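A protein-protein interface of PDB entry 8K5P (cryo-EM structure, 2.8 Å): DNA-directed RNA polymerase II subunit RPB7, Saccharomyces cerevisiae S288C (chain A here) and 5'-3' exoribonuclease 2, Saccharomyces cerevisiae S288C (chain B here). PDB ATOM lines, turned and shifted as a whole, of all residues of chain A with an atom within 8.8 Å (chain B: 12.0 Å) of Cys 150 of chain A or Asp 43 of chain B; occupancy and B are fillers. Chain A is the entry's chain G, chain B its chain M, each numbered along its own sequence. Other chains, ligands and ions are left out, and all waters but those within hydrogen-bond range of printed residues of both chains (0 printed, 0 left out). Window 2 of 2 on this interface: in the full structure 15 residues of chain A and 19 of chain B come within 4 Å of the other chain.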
ATOM      1  N   PRO A  81      20.142   9.626  16.151  1.00  0.00           N
ATOM      2  CA  PRO A  81      18.742  10.017  16.392  1.00  0.00           C
ATOM      3  C   PRO A  81      18.064  10.607  15.168  1.00  0.00           C
ATOM      4  O   PRO A  81      16.861  10.398  14.971  1.00  0.00           O
ATOM      5  CB  PRO A  81      18.855  11.038  17.534  1.00  0.00           C
ATOM      6  CG  PRO A  81      20.271  11.519  17.486  1.00  0.00           C
ATOM      7  CD  PRO A  81      21.081  10.350  17.023  1.00  0.00           C
ATOM      8  N   PHE A  82      18.811  11.345  14.343  1.00  0.00           N
ATOM      9  CA  PHE A  82      18.323  11.897  13.083  1.00  0.00           C
ATOM     10  C   PHE A  82      17.127  12.816  13.328  1.00  0.00           C
ATOM     11  O   PHE A  82      16.875  13.214  14.469  1.00  0.00           O
ATOM     12  CB  PHE A  82      17.967  10.760  12.121  1.00  0.00           C
ATOM     13  CG  PHE A  82      18.467  10.964  10.722  1.00  0.00           C
ATOM     14  CD1 PHE A  82      19.733  10.534  10.365  1.00  0.00           C
ATOM     15  CD2 PHE A  82      17.675  11.564   9.763  1.00  0.00           C
ATOM     16  CE1 PHE A  82      20.207  10.709   9.082  1.00  0.00           C
ATOM     17  CE2 PHE A  82      18.144  11.739   8.476  1.00  0.00           C
ATOM     18  CZ  PHE A  82      19.410  11.313   8.137  1.00  0.00           C
ATOM     19  N   LYS A  83      16.386  13.166  12.277  1.00  0.00           N
ATOM     20  CA  LYS A  83      15.254  14.072  12.440  1.00  0.00           C
ATOM     21  C   LYS A  83      14.286  13.892  11.282  1.00  0.00           C
ATOM     22  O   LYS A  83      14.708  13.838  10.123  1.00  0.00           O
ATOM     23  CB  LYS A  83      15.723  15.530  12.518  1.00  0.00           C
ATOM     24  CG  LYS A  83      14.599  16.535  12.720  1.00  0.00           C
ATOM     25  CD  LYS A  83      15.144  17.929  12.995  1.00  0.00           C
ATOM     26  CE  LYS A  83      14.038  18.973  12.961  1.00  0.00           C
ATOM     27  NZ  LYS A  83      13.371  19.032  11.633  1.00  0.00           N
ATOM     28  N   THR A 111       8.001  17.449  25.927  1.00  0.00           N
ATOM     29  CA  THR A 111       7.684  18.572  26.793  1.00  0.00           C
ATOM     30  C   THR A 111       6.173  18.787  26.855  1.00  0.00           C
ATOM     31  O   THR A 111       5.388  18.068  26.232  1.00  0.00           O
ATOM     32  CB  THR A 111       8.396  19.836  26.313  1.00  0.00           C
ATOM     33  OG1 THR A 111       7.565  20.526  25.372  1.00  0.00           O
ATOM     34  CG2 THR A 111       9.716  19.479  25.646  1.00  0.00           C
ATOM     35  N   HIS A 113       4.261  21.317  25.760  1.00  0.00           N
ATOM     36  CA  HIS A 113       3.642  21.850  24.554  1.00  0.00           C
ATOM     37  C   HIS A 113       3.843  20.950  23.339  1.00  0.00           C
ATOM     38  O   HIS A 113       3.646  21.402  22.206  1.00  0.00           O
ATOM     39  CB  HIS A 113       4.174  23.256  24.266  1.00  0.00           C
ATOM     40  CG  HIS A 113       5.554  23.276  23.686  1.00  0.00           C
ATOM     41  ND1 HIS A 113       5.790  23.278  22.328  1.00  0.00           N
ATOM     42  CD2 HIS A 113       6.770  23.297  24.279  1.00  0.00           C
ATOM     43  CE1 HIS A 113       7.093  23.299  22.110  1.00  0.00           C
ATOM     44  NE2 HIS A 113       7.711  23.310  23.278  1.00  0.00           N
ATOM     45  N   LEU A 114       4.226  19.690  23.549  1.00  0.00           N
ATOM     46  CA  LEU A 114       4.443  18.751  22.454  1.00  0.00           C
ATOM     47  C   LEU A 114       3.255  17.814  22.264  1.00  0.00           C
ATOM     48  O   LEU A 114       2.691  17.736  21.168  1.00  0.00           O
ATOM     49  CB  LEU A 114       5.728  17.948  22.699  1.00  0.00           C
ATOM     50  CG  LEU A 114       6.955  18.393  21.899  1.00  0.00           C
ATOM     51  CD1 LEU A 114       6.694  18.275  20.409  1.00  0.00           C
ATOM     52  CD2 LEU A 114       7.355  19.811  22.260  1.00  0.00           C
ATOM     53  N   ILE A 147      10.053  12.152  16.076  1.00  0.00           N
ATOM     54  CA  ILE A 147      11.136  12.994  16.571  1.00  0.00           C
ATOM     55  C   ILE A 147      11.212  14.265  15.739  1.00  0.00           C
ATOM     56  O   ILE A 147      11.264  14.212  14.504  1.00  0.00           O
ATOM     57  CB  ILE A 147      12.475  12.239  16.542  1.00  0.00           C
ATOM     58  CG1 ILE A 147      12.300  10.819  17.083  1.00  0.00           C
ATOM     59  CG2 ILE A 147      13.528  12.991  17.340  1.00  0.00           C
ATOM     60  CD1 ILE A 147      11.931  10.765  18.549  1.00  0.00           C
ATOM     61  N   GLU A 148      11.220  15.417  16.419  1.00  0.00           N
ATOM     62  CA  GLU A 148      11.387  16.710  15.767  1.00  0.00           C
ATOM     63  C   GLU A 148      12.377  17.597  16.514  1.00  0.00           C
ATOM     64  O   GLU A 148      12.406  18.811  16.289  1.00  0.00           O
ATOM     65  CB  GLU A 148      10.044  17.431  15.627  1.00  0.00           C
ATOM     66  CG  GLU A 148       9.207  16.969  14.448  1.00  0.00           C
ATOM     67  CD  GLU A 148       7.959  16.229  14.880  1.00  0.00           C
ATOM     68  OE1 GLU A 148       7.991  15.589  15.952  1.00  0.00           O
ATOM     69  OE2 GLU A 148       6.948  16.287  14.150  1.00  0.00           O
ATOM     70  N   GLY A 149      13.186  17.019  17.396  1.00  0.00           N
ATOM     71  CA  GLY A 149      14.122  17.801  18.173  1.00  0.00           C
ATOM     72  C   GLY A 149      15.305  18.283  17.355  1.00  0.00           C
ATOM     73  O   GLY A 149      15.565  17.838  16.237  1.00  0.00           O
ATOM     74  N   CYS A 150      16.041  19.223  17.943  1.00  0.00           N
ATOM     75  CA  CYS A 150      17.221  19.799  17.315  1.00  0.00           C
ATOM     76  C   CYS A 150      18.496  19.031  17.637  1.00  0.00           C
ATOM     77  O   CYS A 150      19.584  19.482  17.259  1.00  0.00           O
ATOM     78  CB  CYS A 150      17.383  21.263  17.733  1.00  0.00           C
ATOM     79  SG  CYS A 150      18.138  22.321  16.475  1.00  0.00           S
ATOM     80  N   ILE A 151      18.387  17.903  18.342  1.00  0.00           N
ATOM     81  CA  ILE A 151      19.502  17.006  18.642  1.00  0.00           C
ATOM     82  C   ILE A 151      20.524  17.687  19.546  1.00  0.00           C
ATOM     83  O   ILE A 151      20.828  17.185  20.635  1.00  0.00           O
ATOM     84  CB  ILE A 151      20.167  16.485  17.352  1.00  0.00           C
ATOM     85  CG1 ILE A 151      19.109  15.972  16.373  1.00  0.00           C
ATOM     86  CG2 ILE A 151      21.157  15.384  17.676  1.00  0.00           C
ATOM     87  CD1 ILE A 151      18.290  14.820  16.908  1.00  0.00           C
ATOM     88  N   SER A 152      21.065  18.824  19.102  1.00  0.00           N
ATOM     89  CA  SER A 152      22.066  19.584  19.852  1.00  0.00           C
ATOM     90  C   SER A 152      23.302  18.727  20.137  1.00  0.00           C
ATOM     91  O   SER A 152      23.631  18.412  21.283  1.00  0.00           O
ATOM     92  CB  SER A 152      21.470  20.152  21.145  1.00  0.00           C
ATOM     93  OG  SER A 152      22.483  20.681  21.984  1.00  0.00           O
ATOM     94  N   GLN A 153      23.985  18.352  19.059  1.00  0.00           N
ATOM     95  CA  GLN A 153      25.144  17.463  19.130  1.00  0.00           C
ATOM     96  C   GLN A 153      26.348  18.240  19.648  1.00  0.00           C
ATOM     97  O   GLN A 153      27.046  18.910  18.884  1.00  0.00           O
ATOM     98  CB  GLN A 153      25.433  16.855  17.763  1.00  0.00           C
ATOM     99  CG  GLN A 153      24.292  16.992  16.769  1.00  0.00           C
ATOM    100  CD  GLN A 153      24.640  16.441  15.399  1.00  0.00           C
ATOM    101  OE1 GLN A 153      25.804  16.437  14.998  1.00  0.00           O
ATOM    102  NE2 GLN A 153      23.631  15.970  14.677  1.00  0.00           N
ATOM    103  N   VAL A 154      26.597  18.153  20.953  1.00  0.00           N
ATOM    104  CA  VAL A 154      27.800  18.709  21.572  1.00  0.00           C
ATOM    105  C   VAL A 154      28.362  17.610  22.474  1.00  0.00           C
ATOM    106  O   VAL A 154      27.930  17.436  23.619  1.00  0.00           O
ATOM    107  CB  VAL A 154      27.527  20.003  22.350  1.00  0.00           C
ATOM    108  CG1 VAL A 154      26.220  19.912  23.140  1.00  0.00           C
ATOM    109  CG2 VAL A 154      28.708  20.372  23.246  1.00  0.00           C
ATOM    110  N   SER A 156      27.622  14.798  22.628  1.00  0.00           N
ATOM    111  CA  SER A 156      26.515  13.910  22.955  1.00  0.00           C
ATOM    112  C   SER A 156      25.290  14.398  22.199  1.00  0.00           C
ATOM    113  O   SER A 156      25.145  15.597  21.947  1.00  0.00           O
ATOM    114  CB  SER A 156      26.234  13.878  24.464  1.00  0.00           C
ATOM    115  OG  SER A 156      25.896  15.167  24.949  1.00  0.00           O
ATOM    116  N   ILE A 157      24.414  13.466  21.843  1.00  0.00           N
ATOM    117  CA  ILE A 157      23.208  13.795  21.097  1.00  0.00           C
ATOM    118  C   ILE A 157      21.973  13.530  21.953  1.00  0.00           C
ATOM    119  O   ILE A 157      22.007  12.793  22.943  1.00  0.00           O
ATOM    120  CB  ILE A 157      23.160  13.066  19.726  1.00  0.00           C
ATOM    121  CG1 ILE A 157      23.347  11.535  19.801  1.00  0.00           C
ATOM    122  CG2 ILE A 157      24.202  13.647  18.786  1.00  0.00           C
ATOM    123  CD1 ILE A 157      22.423  10.735  20.679  1.00  0.00           C
ATOM    124  N   HIS A 158      20.871  14.178  21.575  1.00  0.00           N
ATOM    125  CA  HIS A 158      19.606  14.069  22.286  1.00  0.00           C
ATOM    126  C   HIS A 158      18.478  14.034  21.265  1.00  0.00           C
ATOM    127  O   HIS A 158      18.710  14.069  20.052  1.00  0.00           O
ATOM    128  CB  HIS A 158      19.420  15.225  23.279  1.00  0.00           C
ATOM    129  CG  HIS A 158      20.668  15.596  24.016  1.00  0.00           C
ATOM    130  ND1 HIS A 158      21.254  14.769  24.950  1.00  0.00           N
ATOM    131  CD2 HIS A 158      21.446  16.702  23.953  1.00  0.00           C
ATOM    132  CE1 HIS A 158      22.336  15.351  25.433  1.00  0.00           C
ATOM    133  NE2 HIS A 158      22.475  16.525  24.845  1.00  0.00           N
ATOM    134  N   ALA A 159      17.244  13.962  21.759  1.00  0.00           N
ATOM    135  CA  ALA A 159      16.086  13.925  20.878  1.00  0.00           C
ATOM    136  C   ALA A 159      14.867  14.443  21.624  1.00  0.00           C
ATOM    137  O   ALA A 159      14.724  14.232  22.830  1.00  0.00           O
ATOM    138  CB  ALA A 159      15.828  12.510  20.351  1.00  0.00           C
ATOM    139  N   ILE A 160      13.994  15.127  20.887  1.00  0.00           N
ATOM    140  CA  ILE A 160      12.716  15.607  21.398  1.00  0.00           C
ATOM    141  C   ILE A 160      11.619  15.070  20.491  1.00  0.00           C
ATOM    142  O   ILE A 160      11.690  15.224  19.266  1.00  0.00           O
ATOM    143  CB  ILE A 160      12.667  17.145  21.467  1.00  0.00           C
ATOM    144  CG1 ILE A 160      13.722  17.668  22.445  1.00  0.00           C
ATOM    145  CG2 ILE A 160      11.278  17.620  21.866  1.00  0.00           C
ATOM    146  CD1 ILE A 160      13.365  17.460  23.900  1.00  0.00           C
ATOM    147  N   GLY A 161      10.608  14.441  21.090  1.00  0.00           N
ATOM    148  CA  GLY A 161       9.555  13.782  20.353  1.00  0.00           C
ATOM    149  C   GLY A 161       8.215  14.491  20.477  1.00  0.00           C
ATOM    150  O   GLY A 161       7.998  15.342  21.337  1.00  0.00           O
ATOM    151  N   PRO B  39      22.183  20.865  32.439  1.00  0.00           N
ATOM    152  CA  PRO B  39      21.205  20.309  31.496  1.00  0.00           C
ATOM    153  C   PRO B  39      21.149  21.119  30.209  1.00  0.00           C
ATOM    154  O   PRO B  39      21.231  22.349  30.221  1.00  0.00           O
ATOM    155  CB  PRO B  39      19.881  20.384  32.267  1.00  0.00           C
ATOM    156  CG  PRO B  39      20.121  21.370  33.368  1.00  0.00           C
ATOM    157  CD  PRO B  39      21.568  21.249  33.719  1.00  0.00           C
ATOM    158  N   GLN B  40      21.011  20.411  29.093  1.00  0.00           N
ATOM    159  CA  GLN B  40      20.983  21.053  27.786  1.00  0.00           C
ATOM    160  C   GLN B  40      19.640  21.729  27.548  1.00  0.00           C
ATOM    161  O   GLN B  40      18.585  21.198  27.907  1.00  0.00           O
ATOM    162  CB  GLN B  40      21.257  20.030  26.684  1.00  0.00           C
ATOM    163  CG  GLN B  40      22.622  19.365  26.781  1.00  0.00           C
ATOM    164  CD  GLN B  40      22.598  18.101  27.618  1.00  0.00           C
ATOM    165  OE1 GLN B  40      21.600  17.792  28.268  1.00  0.00           O
ATOM    166  NE2 GLN B  40      23.702  17.362  27.605  1.00  0.00           N
ATOM    167  N   ILE B  41      19.686  22.910  26.940  1.00  0.00           N
ATOM    168  CA  ILE B  41      18.494  23.678  26.597  1.00  0.00           C
ATOM    169  C   ILE B  41      18.397  23.737  25.080  1.00  0.00           C
ATOM    170  O   ILE B  41      19.263  24.322  24.417  1.00  0.00           O
ATOM    171  CB  ILE B  41      18.532  25.088  27.205  1.00  0.00           C
ATOM    172  CG1 ILE B  41      18.608  25.009  28.731  1.00  0.00           C
ATOM    173  CG2 ILE B  41      17.315  25.890  26.767  1.00  0.00           C
ATOM    174  CD1 ILE B  41      18.774  26.354  29.403  1.00  0.00           C
ATOM    175  N   VAL B  42      17.348  23.130  24.530  1.00  0.00           N
ATOM    176  CA  VAL B  42      17.121  23.088  23.091  1.00  0.00           C
ATOM    177  C   VAL B  42      15.701  23.559  22.815  1.00  0.00           C
ATOM    178  O   VAL B  42      14.748  23.056  23.422  1.00  0.00           O
ATOM    179  CB  VAL B  42      17.352  21.675  22.519  1.00  0.00           C
ATOM    180  CG1 VAL B  42      17.026  20.621  23.561  1.00  0.00           C
ATOM    181  CG2 VAL B  42      16.528  21.460  21.258  1.00  0.00           C
ATOM    182  N   ASP B  43      15.565  24.527  21.906  1.00  0.00           N
ATOM    183  CA  ASP B  43      14.265  25.073  21.511  1.00  0.00           C
ATOM    184  C   ASP B  43      13.490  25.602  22.717  1.00  0.00           C
ATOM    185  O   ASP B  43      12.269  25.458  22.805  1.00  0.00           O
ATOM    186  CB  ASP B  43      13.440  24.036  20.745  1.00  0.00           C
ATOM    187  CG  ASP B  43      14.162  23.502  19.524  1.00  0.00           C
ATOM    188  OD1 ASP B  43      15.316  23.916  19.286  1.00  0.00           O
ATOM    189  OD2 ASP B  43      13.576  22.668  18.802  1.00  0.00           O
ATOM    190  N   GLY B  44      14.206  26.220  23.653  1.00  0.00           N
ATOM    191  CA  GLY B  44      13.580  26.795  24.826  1.00  0.00           C
ATOM    192  C   GLY B  44      13.356  25.807  25.953  1.00  0.00           C
ATOM    193  O   GLY B  44      13.454  26.168  27.129  1.00  0.00           O
ATOM    194  N   VAL B  45      13.053  24.554  25.606  1.00  0.00           N
ATOM    195  CA  VAL B  45      12.788  23.549  26.630  1.00  0.00           C
ATOM    196  C   VAL B  45      14.088  23.143  27.317  1.00  0.00           C
ATOM    197  O   VAL B  45      15.195  23.339  26.800  1.00  0.00           O
ATOM    198  CB  VAL B  45      12.069  22.331  26.026  1.00  0.00           C
ATOM    199  CG1 VAL B  45      11.178  22.762  24.870  1.00  0.00           C
ATOM    200  CG2 VAL B  45      13.072  21.279  25.571  1.00  0.00           C
ATOM    201  N   ILE B  46      13.947  22.574  28.511  1.00  0.00           N
ATOM    202  CA  ILE B  46      15.077  22.153  29.331  1.00  0.00           C
ATOM    203  C   ILE B  46      15.031  20.637  29.460  1.00  0.00           C
ATOM    204  O   ILE B  46      14.017  20.072  29.889  1.00  0.00           O
ATOM    205  CB  ILE B  46      15.056  22.825  30.712  1.00  0.00           C
ATOM    206  CG1 ILE B  46      15.112  24.346  30.565  1.00  0.00           C
ATOM    207  CG2 ILE B  46      16.212  22.324  31.565  1.00  0.00           C
ATOM    208  CD1 ILE B  46      15.112  25.088  31.883  1.00  0.00           C
ATOM    209  N   LEU B  47      16.124  19.983  29.090  1.00  0.00           N
ATOM    210  CA  LEU B  47      16.195  18.530  29.194  1.00  0.00           C
ATOM    211  C   LEU B  47      16.346  18.119  30.655  1.00  0.00           C
ATOM    212  O   LEU B  47      17.267  18.587  31.333  1.00  0.00           O
ATOM    213  CB  LEU B  47      17.364  17.993  28.372  1.00  0.00           C
ATOM    214  CG  LEU B  47      17.012  17.286  27.064  1.00  0.00           C
ATOM    215  CD1 LEU B  47      16.236  16.010  27.344  1.00  0.00           C
ATOM    216  CD2 LEU B  47      16.215  18.208  26.160  1.00  0.00           C
ATOM    217  N   PRO B  48      15.469  17.258  31.174  1.00  0.00           N
ATOM    218  CA  PRO B  48      15.628  16.778  32.556  1.00  0.00           C
ATOM    219  C   PRO B  48      16.840  15.866  32.666  1.00  0.00           C
ATOM    220  O   PRO B  48      16.941  14.858  31.962  1.00  0.00           O
ATOM    221  CB  PRO B  48      14.320  16.024  32.823  1.00  0.00           C
ATOM    222  CG  PRO B  48      13.835  15.619  31.471  1.00  0.00           C
ATOM    223  CD  PRO B  48      14.272  16.700  30.523  1.00  0.00           C
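Of the 20 printed residues of chain A, 5 touch a printed residue of chain B.
Printed residues of chain A that touch a printed residue of chain B: Thr 111, His 113, Cys 150, His 158 and Ile 160.
Hydrophobic or aromatic side chains of chain A that line the printed part of chain B: His 113, His 158 and Ile 160.
Of the 10 printed residues of chain B, 5 touch a printed residue of chain A.
Printed residues of chain B that touch a printed residue of chain A: Gln 40, Val 42, Asp 43, Val 45 and Leu 47.
Along chain B the printed residues that touch a printed residue of chain A span positions 40 to 47.
Among the printed residues, 6 pairs touch across the chains.
Among the printed residues, no Asp or Glu carboxylate lies within 4 Å of a Lys or Arg side-chain nitrogen of the other chain.
Cys 150 of chain A touches just these residues of chain B: Val 42 (3.6 Å) and Asp 43 (3.7 Å).
Asp 43 of chain B touches just one residue of chain A: Cys 150 (3.7 Å).
No residue of chain B comes within 4 Å of Ile 151 of chain A.
Ser 152 of chain A touches none of the printed residues of chain B.
No residue of chain B comes within 4 Å of Ala 159 of chain A.
Of the printed residues of chain B, Ile 160 of chain A touches Leu 47.
Val 42 of chain B touches just one residue of chain A: Cys 150 (3.6 Å).
No residue of chain A comes within 4 Å of Gly 44 of chain B.
Of the printed residues of chain B, Thr 111 of chain A touches Val 45.
Of the printed residues of chain A, Gln 40 of chain B touches His 158.
Of the printed residues of chain A, Val 45 of chain B touches Thr 111 and His 113.
Of the printed residues of chain A, Leu 47 of chain B touches Ile 160 (3.7 Å).
The nearest residue of chain A that does not touch Asp 43 of chain B is Glu 148 of chain A (4.7 Å).
Among the printed residues, pairs that only touch across the chains: Cys 150 of chain A with Val 42 of chain B, Thr 111 of chain A with Val 45 of chain B, Cys 150 of chain A with Asp 43 of chain B, Ile 160 of chain A with Leu 47 of chain B and His 113 of chain A with Val 45 of chain B.
The side-chain hydroxyl (OG1) of Thr 111 of chain A lies close to the backbone NH (N) of His 113 of chain A (3.4 Å).
O of Ile 160 of chain A lies within hydrogen-bond range of N of Glu 148 of chain A, 2.9 Å away.
The backbone carbonyl oxygen (O) of Ile 160 of chain A lies within hydrogen-bond range of the backbone NH (N) of Gly 149 of chain A, at 3.0 Å.
The backbone carbonyl oxygen (O) of Ile 151 of chain A is in hydrogen-bond range of the backbone NH (N) of His 158 of chain A.
The backbone carbonyl oxygen (O) of Gln 40 of chain B is in hydrogen-bond range of the backbone NH (N) of Leu 47 of chain B, at 3.0 Å.
A ring nitrogen (NE2) of His 158 of chain A lies within hydrogen-bond range of the side-chain amide nitrogen (NE2) of Gln 40 of chain B (3.1 Å).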
